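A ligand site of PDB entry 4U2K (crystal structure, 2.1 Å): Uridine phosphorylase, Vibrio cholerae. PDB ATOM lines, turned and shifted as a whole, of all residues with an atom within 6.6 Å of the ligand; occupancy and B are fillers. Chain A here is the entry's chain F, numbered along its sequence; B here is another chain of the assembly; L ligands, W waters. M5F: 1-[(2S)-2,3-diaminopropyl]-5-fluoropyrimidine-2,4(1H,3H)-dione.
NE2 of His 7 of chain B is in hydrogen-bond range of NAJ of the ligand (2.6 Å).
The guanidinium group (NH2) of Arg 167 sits at hydrogen-bond distance from an oxygen (O4) of the ligand (2.9 Å).
The side-chain amide oxygen of Gln 165 sits at hydrogen-bond distance from a nitrogen (N3) of the ligand.
The side-chain sulfur (SD) of Met 196 is in hydrogen-bond range of a nitrogen (NAA) of the ligand (3.1 Å).
Water W2 lies within hydrogen-bond range of an oxygen (O4) of the ligand, the guanidinium group of Arg 167, the guanidinium group of Arg 222 and the side-chain amide oxygen of Gln 165.
Water W4 lies within hydrogen-bond range of OE2 of Glu 197 (2.4 Å) and NAA of the ligand (2.6 Å).
Water W3 lies within hydrogen-bond range of NAJ of the ligand (2.7 Å) and NE2 of His 7 of chain B (3.1 Å).
Water W1 lies within hydrogen-bond range of the side-chain carboxylate (OE1) of Glu 197, a nitrogen (NAA) of the ligand and the backbone NH (N) of Met 196.
Thr 93 touches the ligand.
Gly 95 touches the ligand.
Phe 161 touches the ligand (CD2 to CAL, 3.4 Å).
Phe 194 touches the ligand.
Glu 195 touches the ligand (CA to O2, 3.4 Å).
CD1 of Ile 219 touches F5 of the ligand, 3.7 Å away.
CG2 of Ile 220 touches F5 of the ligand, at 3.5 Å.
Phe 6 of chain B touches the ligand.
Hydrophobic or aromatic side chains within 4 Å of the ligand: Phe 161, Met 196, Ile 219, Ile 220, Phe 6 of chain B and His 7 of chain B.
Within 4 Å of the ligand: Thr 93, Gly 95, Phe 161, Gln 165, Arg 167, Phe 194, Glu 195, Met 196, Ile 219, Ile 220, Phe 6 of chain B and His 7 of chain B.
The nearest printed residue that does not touch the ligand is Thr 94 (4.1 Å).
NH1 of Arg 167 sits at hydrogen-bond distance from OE1 of Gln 165, at 2.9 Å.
The guanidinium group (NH1) of Arg 167 sits at hydrogen-bond distance from the backbone carbonyl oxygen (O) of Phe 161, 3.0 Å away.
The backbone carbonyl oxygen (O) of Gln 165 lies within hydrogen-bond range of the guanidinium group (NH2) of Arg 222, 2.8 Å away.
The side-chain amide nitrogen (NE2) of Gln 165 is in hydrogen-bond range of the backbone carbonyl oxygen (O) of Thr 160 (3.2 Å).
O of Glu 195 lies within hydrogen-bond range of N of Ser 158, at 2.8 Å.
The backbone NH (N) of Ala 96 is in hydrogen-bond range of the backbone carbonyl oxygen (O) of Ile 220 (2.8 Å).
The backbone NH (N) of Ile 219 lies within hydrogen-bond range of the backbone carbonyl oxygen (O) of Thr 94, at 3.0 Å.
The side-chain hydroxyl (OG1) of Thr 94 is in hydrogen-bond range of the backbone carbonyl oxygen (O) of Phe 194 (2.5 Å).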
ATOM      1  N   ILE A  68      -2.070   1.904  -0.490  1.00  0.00           N
ATOM      2  CA  ILE A  68      -2.377   3.238   0.019  1.00  0.00           C
ATOM      3  C   ILE A  68      -3.574   3.301   0.957  1.00  0.00           C
ATOM      4  O   ILE A  68      -4.661   2.859   0.611  1.00  0.00           O
ATOM      5  CB  ILE A  68      -2.592   4.254  -1.126  1.00  0.00           C
ATOM      6  CG1 ILE A  68      -1.252   4.543  -1.806  1.00  0.00           C
ATOM      7  CG2 ILE A  68      -3.279   5.544  -0.600  1.00  0.00           C
ATOM      8  CD1 ILE A  68      -1.231   4.135  -3.229  1.00  0.00           C
ATOM      9  N   GLY A  69      -3.349   3.835   2.159  1.00  0.00           N
ATOM     10  CA  GLY A  69      -4.435   4.097   3.083  1.00  0.00           C
ATOM     11  C   GLY A  69      -4.504   3.184   4.300  1.00  0.00           C
ATOM     12  O   GLY A  69      -4.087   2.028   4.270  1.00  0.00           O
ATOM     13  N   ARG A  90       7.065   1.990   9.332  1.00  0.00           N
ATOM     14  CA  ARG A  90       6.537   2.594   8.132  1.00  0.00           C
ATOM     15  C   ARG A  90       7.578   3.550   7.549  1.00  0.00           C
ATOM     16  O   ARG A  90       8.084   4.407   8.246  1.00  0.00           O
ATOM     17  CB  ARG A  90       5.258   3.372   8.473  1.00  0.00           C
ATOM     18  CG  ARG A  90       4.722   4.208   7.377  1.00  0.00           C
ATOM     19  CD  ARG A  90       3.886   3.380   6.447  1.00  0.00           C
ATOM     20  NE  ARG A  90       3.618   4.105   5.215  1.00  0.00           N
ATOM     21  CZ  ARG A  90       2.981   3.571   4.182  1.00  0.00           C
ATOM     22  NH1 ARG A  90       2.558   2.308   4.266  1.00  0.00           N
ATOM     23  NH2 ARG A  90       2.773   4.279   3.094  1.00  0.00           N
ATOM     24  N   THR A  93       7.195   8.666   1.585  1.00  0.00           N
ATOM     25  CA  THR A  93       7.389  10.067   1.231  1.00  0.00           C
ATOM     26  C   THR A  93       6.260  10.904   1.829  1.00  0.00           C
ATOM     27  O   THR A  93       5.164  10.401   2.154  1.00  0.00           O
ATOM     28  CB  THR A  93       7.403  10.278  -0.273  1.00  0.00           C
ATOM     29  OG1 THR A  93       6.111   9.964  -0.812  1.00  0.00           O
ATOM     30  CG2 THR A  93       8.461   9.384  -0.940  1.00  0.00           C
ATOM     31  N   THR A  94       6.540  12.190   1.962  1.00  0.00           N
ATOM     32  CA  THR A  94       5.588  13.101   2.556  1.00  0.00           C
ATOM     33  C   THR A  94       5.767  14.507   2.014  1.00  0.00           C
ATOM     34  O   THR A  94       6.827  14.841   1.491  1.00  0.00           O
ATOM     35  CB  THR A  94       5.721  13.099   4.079  1.00  0.00           C
ATOM     36  OG1 THR A  94       4.594  13.765   4.661  1.00  0.00           O
ATOM     37  CG2 THR A  94       7.016  13.771   4.509  1.00  0.00           C
ATOM     38  N   GLY A  95       4.739  15.319   2.138  1.00  0.00           N
ATOM     39  CA  GLY A  95       4.850  16.720   1.794  1.00  0.00           C
ATOM     40  C   GLY A  95       4.841  17.575   3.041  1.00  0.00           C
ATOM     41  O   GLY A  95       3.946  17.449   3.886  1.00  0.00           O
ATOM     42  N   ALA A  96       5.828  18.472   3.137  1.00  0.00           N
ATOM     43  CA  ALA A  96       5.997  19.330   4.313  1.00  0.00           C
ATOM     44  C   ALA A  96       5.145  20.585   4.217  1.00  0.00           C
ATOM     45  O   ALA A  96       4.873  21.085   3.124  1.00  0.00           O
ATOM     46  CB  ALA A  96       7.468  19.681   4.506  1.00  0.00           C
ATOM     47  N   SER A 158      -4.204  11.752   6.618  1.00  0.00           N
ATOM     48  CA  SER A 158      -5.478  11.966   5.947  1.00  0.00           C
ATOM     49  C   SER A 158      -5.899  10.748   5.135  1.00  0.00           C
ATOM     50  O   SER A 158      -5.062  10.080   4.513  1.00  0.00           O
ATOM     51  CB  SER A 158      -5.347  13.185   5.001  1.00  0.00           C
ATOM     52  OG  SER A 158      -6.442  13.283   4.106  1.00  0.00           O
ATOM     53  N   THR A 160      -7.625  10.996   2.569  1.00  0.00           N
ATOM     54  CA  THR A 160      -7.525  11.428   1.166  1.00  0.00           C
ATOM     55  C   THR A 160      -6.207  12.160   0.927  1.00  0.00           C
ATOM     56  O   THR A 160      -5.608  12.675   1.866  1.00  0.00           O
ATOM     57  CB  THR A 160      -8.664  12.380   0.734  1.00  0.00           C
ATOM     58  OG1 THR A 160      -8.716  13.481   1.647  1.00  0.00           O
ATOM     59  CG2 THR A 160      -9.997  11.690   0.746  1.00  0.00           C
ATOM     60  N   PHE A 161      -5.805  12.205  -0.337  1.00  0.00           N
ATOM     61  CA  PHE A 161      -4.609  12.923  -0.780  1.00  0.00           C
ATOM     62  C   PHE A 161      -5.031  14.309  -1.225  1.00  0.00           C
ATOM     63  O   PHE A 161      -4.224  15.221  -1.260  1.00  0.00           O
ATOM     64  CB  PHE A 161      -3.980  12.163  -1.957  1.00  0.00           C
ATOM     65  CG  PHE A 161      -2.816  12.878  -2.610  1.00  0.00           C
ATOM     66  CD1 PHE A 161      -3.021  13.752  -3.670  1.00  0.00           C
ATOM     67  CD2 PHE A 161      -1.518  12.647  -2.174  1.00  0.00           C
ATOM     68  CE1 PHE A 161      -1.948  14.386  -4.276  1.00  0.00           C
ATOM     69  CE2 PHE A 161      -0.445  13.282  -2.779  1.00  0.00           C
ATOM     70  CZ  PHE A 161      -0.660  14.151  -3.830  1.00  0.00           C
ATOM     71  N   GLN A 165      -6.187  17.152   2.511  1.00  0.00           N
ATOM     72  CA  GLN A 165      -4.897  17.838   2.559  1.00  0.00           C
ATOM     73  C   GLN A 165      -5.046  19.206   1.875  1.00  0.00           C
ATOM     74  O   GLN A 165      -4.067  19.815   1.441  1.00  0.00           O
ATOM     75  CB  GLN A 165      -3.813  17.017   1.845  1.00  0.00           C
ATOM     76  CG  GLN A 165      -3.838  15.540   2.257  1.00  0.00           C
ATOM     77  CD  GLN A 165      -2.587  14.804   1.895  1.00  0.00           C
ATOM     78  OE1 GLN A 165      -1.629  15.403   1.390  1.00  0.00           O
ATOM     79  NE2 GLN A 165      -2.558  13.497   2.151  1.00  0.00           N
ATOM     80  N   ARG A 167      -6.271  20.363  -1.136  1.00  0.00           N
ATOM     81  CA  ARG A 167      -5.837  20.631  -2.509  1.00  0.00           C
ATOM     82  C   ARG A 167      -7.044  21.076  -3.303  1.00  0.00           C
ATOM     83  O   ARG A 167      -8.096  20.448  -3.253  1.00  0.00           O
ATOM     84  CB  ARG A 167      -5.237  19.369  -3.149  1.00  0.00           C
ATOM     85  CG  ARG A 167      -3.993  18.853  -2.448  1.00  0.00           C
ATOM     86  CD  ARG A 167      -3.354  17.677  -3.189  1.00  0.00           C
ATOM     87  NE  ARG A 167      -1.898  17.831  -3.174  1.00  0.00           N
ATOM     88  CZ  ARG A 167      -1.126  17.430  -2.183  1.00  0.00           C
ATOM     89  NH1 ARG A 167      -1.679  16.811  -1.140  1.00  0.00           N
ATOM     90  NH2 ARG A 167       0.191  17.628  -2.209  1.00  0.00           N
ATOM     91  N   PHE A 194       2.020  16.263   5.725  1.00  0.00           N
ATOM     92  CA  PHE A 194       0.875  15.414   5.457  1.00  0.00           C
ATOM     93  C   PHE A 194       1.295  14.039   4.943  1.00  0.00           C
ATOM     94  O   PHE A 194       2.194  13.964   4.092  1.00  0.00           O
ATOM     95  CB  PHE A 194       0.000  16.015   4.365  1.00  0.00           C
ATOM     96  CG  PHE A 194      -1.047  16.973   4.856  1.00  0.00           C
ATOM     97  CD1 PHE A 194      -2.030  16.573   5.738  1.00  0.00           C
ATOM     98  CD2 PHE A 194      -1.080  18.266   4.360  1.00  0.00           C
ATOM     99  CE1 PHE A 194      -3.009  17.452   6.155  1.00  0.00           C
ATOM    100  CE2 PHE A 194      -2.073  19.162   4.781  1.00  0.00           C
ATOM    101  CZ  PHE A 194      -3.032  18.742   5.678  1.00  0.00           C
ATOM    102  N   GLU A 195       0.620  12.987   5.415  1.00  0.00           N
ATOM    103  CA  GLU A 195       0.642  11.704   4.710  1.00  0.00           C
ATOM    104  C   GLU A 195      -0.636  10.873   4.956  1.00  0.00           C
ATOM    105  O   GLU A 195      -1.631  11.374   5.525  1.00  0.00           O
ATOM    106  CB  GLU A 195       1.921  10.892   5.011  1.00  0.00           C
ATOM    107  CG  GLU A 195       2.208  10.602   6.473  1.00  0.00           C
ATOM    108  CD  GLU A 195       1.217   9.640   7.086  1.00  0.00           C
ATOM    109  OE1 GLU A 195       1.367   8.396   6.911  1.00  0.00           O
ATOM    110  OE2 GLU A 195       0.267  10.131   7.742  1.00  0.00           O
ATOM    111  N   MET A 196      -0.643   9.614   4.539  1.00  0.00           N
ATOM    112  CA  MET A 196      -1.940   8.956   4.473  1.00  0.00           C
ATOM    113  C   MET A 196      -2.145   7.748   5.367  1.00  0.00           C
ATOM    114  O   MET A 196      -3.265   7.229   5.441  1.00  0.00           O
ATOM    115  CB  MET A 196      -2.320   8.650   3.029  1.00  0.00           C
ATOM    116  CG  MET A 196      -2.475   9.926   2.173  1.00  0.00           C
ATOM    117  SD  MET A 196      -3.026   9.520   0.516  1.00  0.00           S
ATOM    118  CE  MET A 196      -4.742   9.118   0.791  1.00  0.00           C
ATOM    119  N   GLU A 197      -1.098   7.281   6.055  1.00  0.00           N
ATOM    120  CA  GLU A 197      -1.198   5.984   6.745  1.00  0.00           C
ATOM    121  C   GLU A 197      -0.805   5.978   8.218  1.00  0.00           C
ATOM    122  O   GLU A 197      -1.132   5.021   8.927  1.00  0.00           O
ATOM    123  CB  GLU A 197      -0.393   4.894   6.016  1.00  0.00           C
ATOM    124  CG  GLU A 197      -0.988   4.388   4.691  1.00  0.00           C
ATOM    125  CD  GLU A 197      -0.557   5.228   3.514  1.00  0.00           C
ATOM    126  OE1 GLU A 197       0.335   6.067   3.677  1.00  0.00           O
ATOM    127  OE2 GLU A 197      -1.112   5.042   2.408  1.00  0.00           O
ATOM    128  N   ILE A 219       9.328  15.230  -0.122  1.00  0.00           N
ATOM    129  CA  ILE A 219       9.499  15.320  -1.569  1.00  0.00           C
ATOM    130  C   ILE A 219       8.826  16.571  -2.153  1.00  0.00           C
ATOM    131  O   ILE A 219       8.828  16.774  -3.356  1.00  0.00           O
ATOM    132  CB  ILE A 219       8.954  14.085  -2.293  1.00  0.00           C
ATOM    133  CG1 ILE A 219       7.433  14.021  -2.149  1.00  0.00           C
ATOM    134  CG2 ILE A 219       9.627  12.842  -1.738  1.00  0.00           C
ATOM    135  CD1 ILE A 219       6.764  12.961  -2.988  1.00  0.00           C
ATOM    136  N   ILE A 220       8.237  17.375  -1.284  1.00  0.00           N
ATOM    137  CA  ILE A 220       7.569  18.601  -1.678  1.00  0.00           C
ATOM    138  C   ILE A 220       7.298  19.443  -0.437  1.00  0.00           C
ATOM    139  O   ILE A 220       7.107  18.923   0.661  1.00  0.00           O
ATOM    140  CB  ILE A 220       6.246  18.306  -2.450  1.00  0.00           C
ATOM    141  CG1 ILE A 220       5.579  19.610  -2.914  1.00  0.00           C
ATOM    142  CG2 ILE A 220       5.296  17.484  -1.605  1.00  0.00           C
ATOM    143  CD1 ILE A 220       4.195  19.415  -3.506  1.00  0.00           C
ATOM    144  N   ARG A 222       4.702  22.579   0.275  1.00  0.00           N
ATOM    145  CA  ARG A 222       3.627  23.379  -0.281  1.00  0.00           C
ATOM    146  C   ARG A 222       3.878  24.879  -0.087  1.00  0.00           C
ATOM    147  O   ARG A 222       3.301  25.705  -0.795  1.00  0.00           O
ATOM    148  CB  ARG A 222       2.292  22.990   0.367  1.00  0.00           C
ATOM    149  CG  ARG A 222       2.099  21.486   0.616  1.00  0.00           C
ATOM    150  CD  ARG A 222       1.159  20.834  -0.418  1.00  0.00           C
ATOM    151  NE  ARG A 222      -0.135  21.517  -0.555  1.00  0.00           N
ATOM    152  CZ  ARG A 222      -1.290  21.084  -0.040  1.00  0.00           C
ATOM    153  NH1 ARG A 222      -2.407  21.802  -0.232  1.00  0.00           N
ATOM    154  NH2 ARG A 222      -1.341  19.959   0.666  1.00  0.00           N
ATOM    155  N   PHE B   6      -0.963  12.231 -11.019  1.00  0.00           N
ATOM    156  CA  PHE B   6       0.087  11.912 -10.061  1.00  0.00           C
ATOM    157  C   PHE B   6       0.242  10.415  -9.739  1.00  0.00           C
ATOM    158  O   PHE B   6       1.368   9.942  -9.605  1.00  0.00           O
ATOM    159  CB  PHE B   6      -0.111  12.741  -8.791  1.00  0.00           C
ATOM    160  CG  PHE B   6       1.063  12.689  -7.843  1.00  0.00           C
ATOM    161  CD1 PHE B   6       2.120  13.575  -7.994  1.00  0.00           C
ATOM    162  CD2 PHE B   6       1.095  11.757  -6.812  1.00  0.00           C
ATOM    163  CE1 PHE B   6       3.203  13.526  -7.121  1.00  0.00           C
ATOM    164  CE2 PHE B   6       2.164  11.710  -5.943  1.00  0.00           C
ATOM    165  CZ  PHE B   6       3.229  12.591  -6.098  1.00  0.00           C
ATOM    166  N   HIS B   7      -0.861   9.679  -9.609  1.00  0.00           N
ATOM    167  CA  HIS B   7      -0.785   8.255  -9.228  1.00  0.00           C
ATOM    168  C   HIS B   7      -1.022   7.227 -10.341  1.00  0.00           C
ATOM    169  O   HIS B   7      -0.290   6.255 -10.457  1.00  0.00           O
ATOM    170  CB  HIS B   7      -1.733   7.947  -8.079  1.00  0.00           C
ATOM    171  CG  HIS B   7      -1.406   8.685  -6.821  1.00  0.00           C
ATOM    172  ND1 HIS B   7      -1.920   9.926  -6.526  1.00  0.00           N
ATOM    173  CD2 HIS B   7      -0.583   8.362  -5.793  1.00  0.00           C
ATOM    174  CE1 HIS B   7      -1.448  10.332  -5.372  1.00  0.00           C
ATOM    175  NE2 HIS B   7      -0.629   9.404  -4.902  1.00  0.00           N
ATOM    176  N   ARG B  47       1.570   0.902  -8.553  1.00  0.00           N
ATOM    177  CA  ARG B  47       1.018   0.468  -7.278  1.00  0.00           C
ATOM    178  C   ARG B  47      -0.148  -0.483  -7.505  1.00  0.00           C
ATOM    179  O   ARG B  47       0.015  -1.520  -8.147  1.00  0.00           O
ATOM    180  CB  ARG B  47       0.614   1.670  -6.411  1.00  0.00           C
ATOM    181  CG  ARG B  47       1.791   2.620  -6.139  1.00  0.00           C
ATOM    182  CD  ARG B  47       1.331   3.953  -5.565  1.00  0.00           C
ATOM    183  NE  ARG B  47       2.413   4.664  -4.897  1.00  0.00           N
ATOM    184  CZ  ARG B  47       2.718   4.535  -3.600  1.00  0.00           C
ATOM    185  NH1 ARG B  47       2.004   3.712  -2.830  1.00  0.00           N
ATOM    186  NH2 ARG B  47       3.723   5.215  -3.085  1.00  0.00           N
ATOM    187  N   ILE B  75      -8.360   8.336  -4.645  1.00  0.00           N
ATOM    188  CA  ILE B  75      -7.311   8.735  -5.564  1.00  0.00           C
ATOM    189  C   ILE B  75      -7.631   8.340  -7.020  1.00  0.00           C
ATOM    190  O   ILE B  75      -7.561   9.173  -7.934  1.00  0.00           O
ATOM    191  CB  ILE B  75      -5.964   8.138  -5.120  1.00  0.00           C
ATOM    192  CG1 ILE B  75      -5.472   8.851  -3.861  1.00  0.00           C
ATOM    193  CG2 ILE B  75      -4.946   8.175  -6.248  1.00  0.00           C
ATOM    194  CD1 ILE B  75      -4.224   8.219  -3.223  1.00  0.00           C
HETATM  195  F5  M5F L   1       3.703  14.368  -1.488  1.00  0.00           F
HETATM  196  C5  M5F L   1       2.796  13.765  -0.797  1.00  0.00           C
HETATM  197  C6  M5F L   1       2.910  12.342  -0.550  1.00  0.00           C
HETATM  198  N1  M5F L   1       1.975  11.773   0.149  1.00  0.00           N
HETATM  199  CAB M5F L   1       2.032  10.300   0.431  1.00  0.00           C
HETATM  200  CAM M5F L   1       1.243   9.464  -0.452  1.00  0.00           C
HETATM  201  CAL M5F L   1       0.840  10.242  -1.706  1.00  0.00           C
HETATM  202  NAJ M5F L   1       1.080   9.558  -2.905  1.00  0.00           N
HETATM  203  NAA M5F L   1       0.008   9.074   0.173  1.00  0.00           N
HETATM  204  C2  M5F L   1       0.907  12.488   0.654  1.00  0.00           C
HETATM  205  O2  M5F L   1       0.014  11.868   1.341  1.00  0.00           O
HETATM  206  N3  M5F L   1       0.802  13.776   0.438  1.00  0.00           N
HETATM  207  C4  M5F L   1       1.748  14.450  -0.296  1.00  0.00           C
HETATM  208  O4  M5F L   1       1.614  15.811  -0.518  1.00  0.00           O
HETATM  209  O   HOH W   1       1.025   8.418   2.631  1.00  0.00           O
HETATM  210  O   HOH W   2       0.955  17.593   1.009  1.00  0.00           O
HETATM  211  O   HOH W   3       0.227   7.004  -3.217  1.00  0.00           O
HETATM  212  O   HOH W   4       0.122   6.649   1.055  1.00  0.00           O
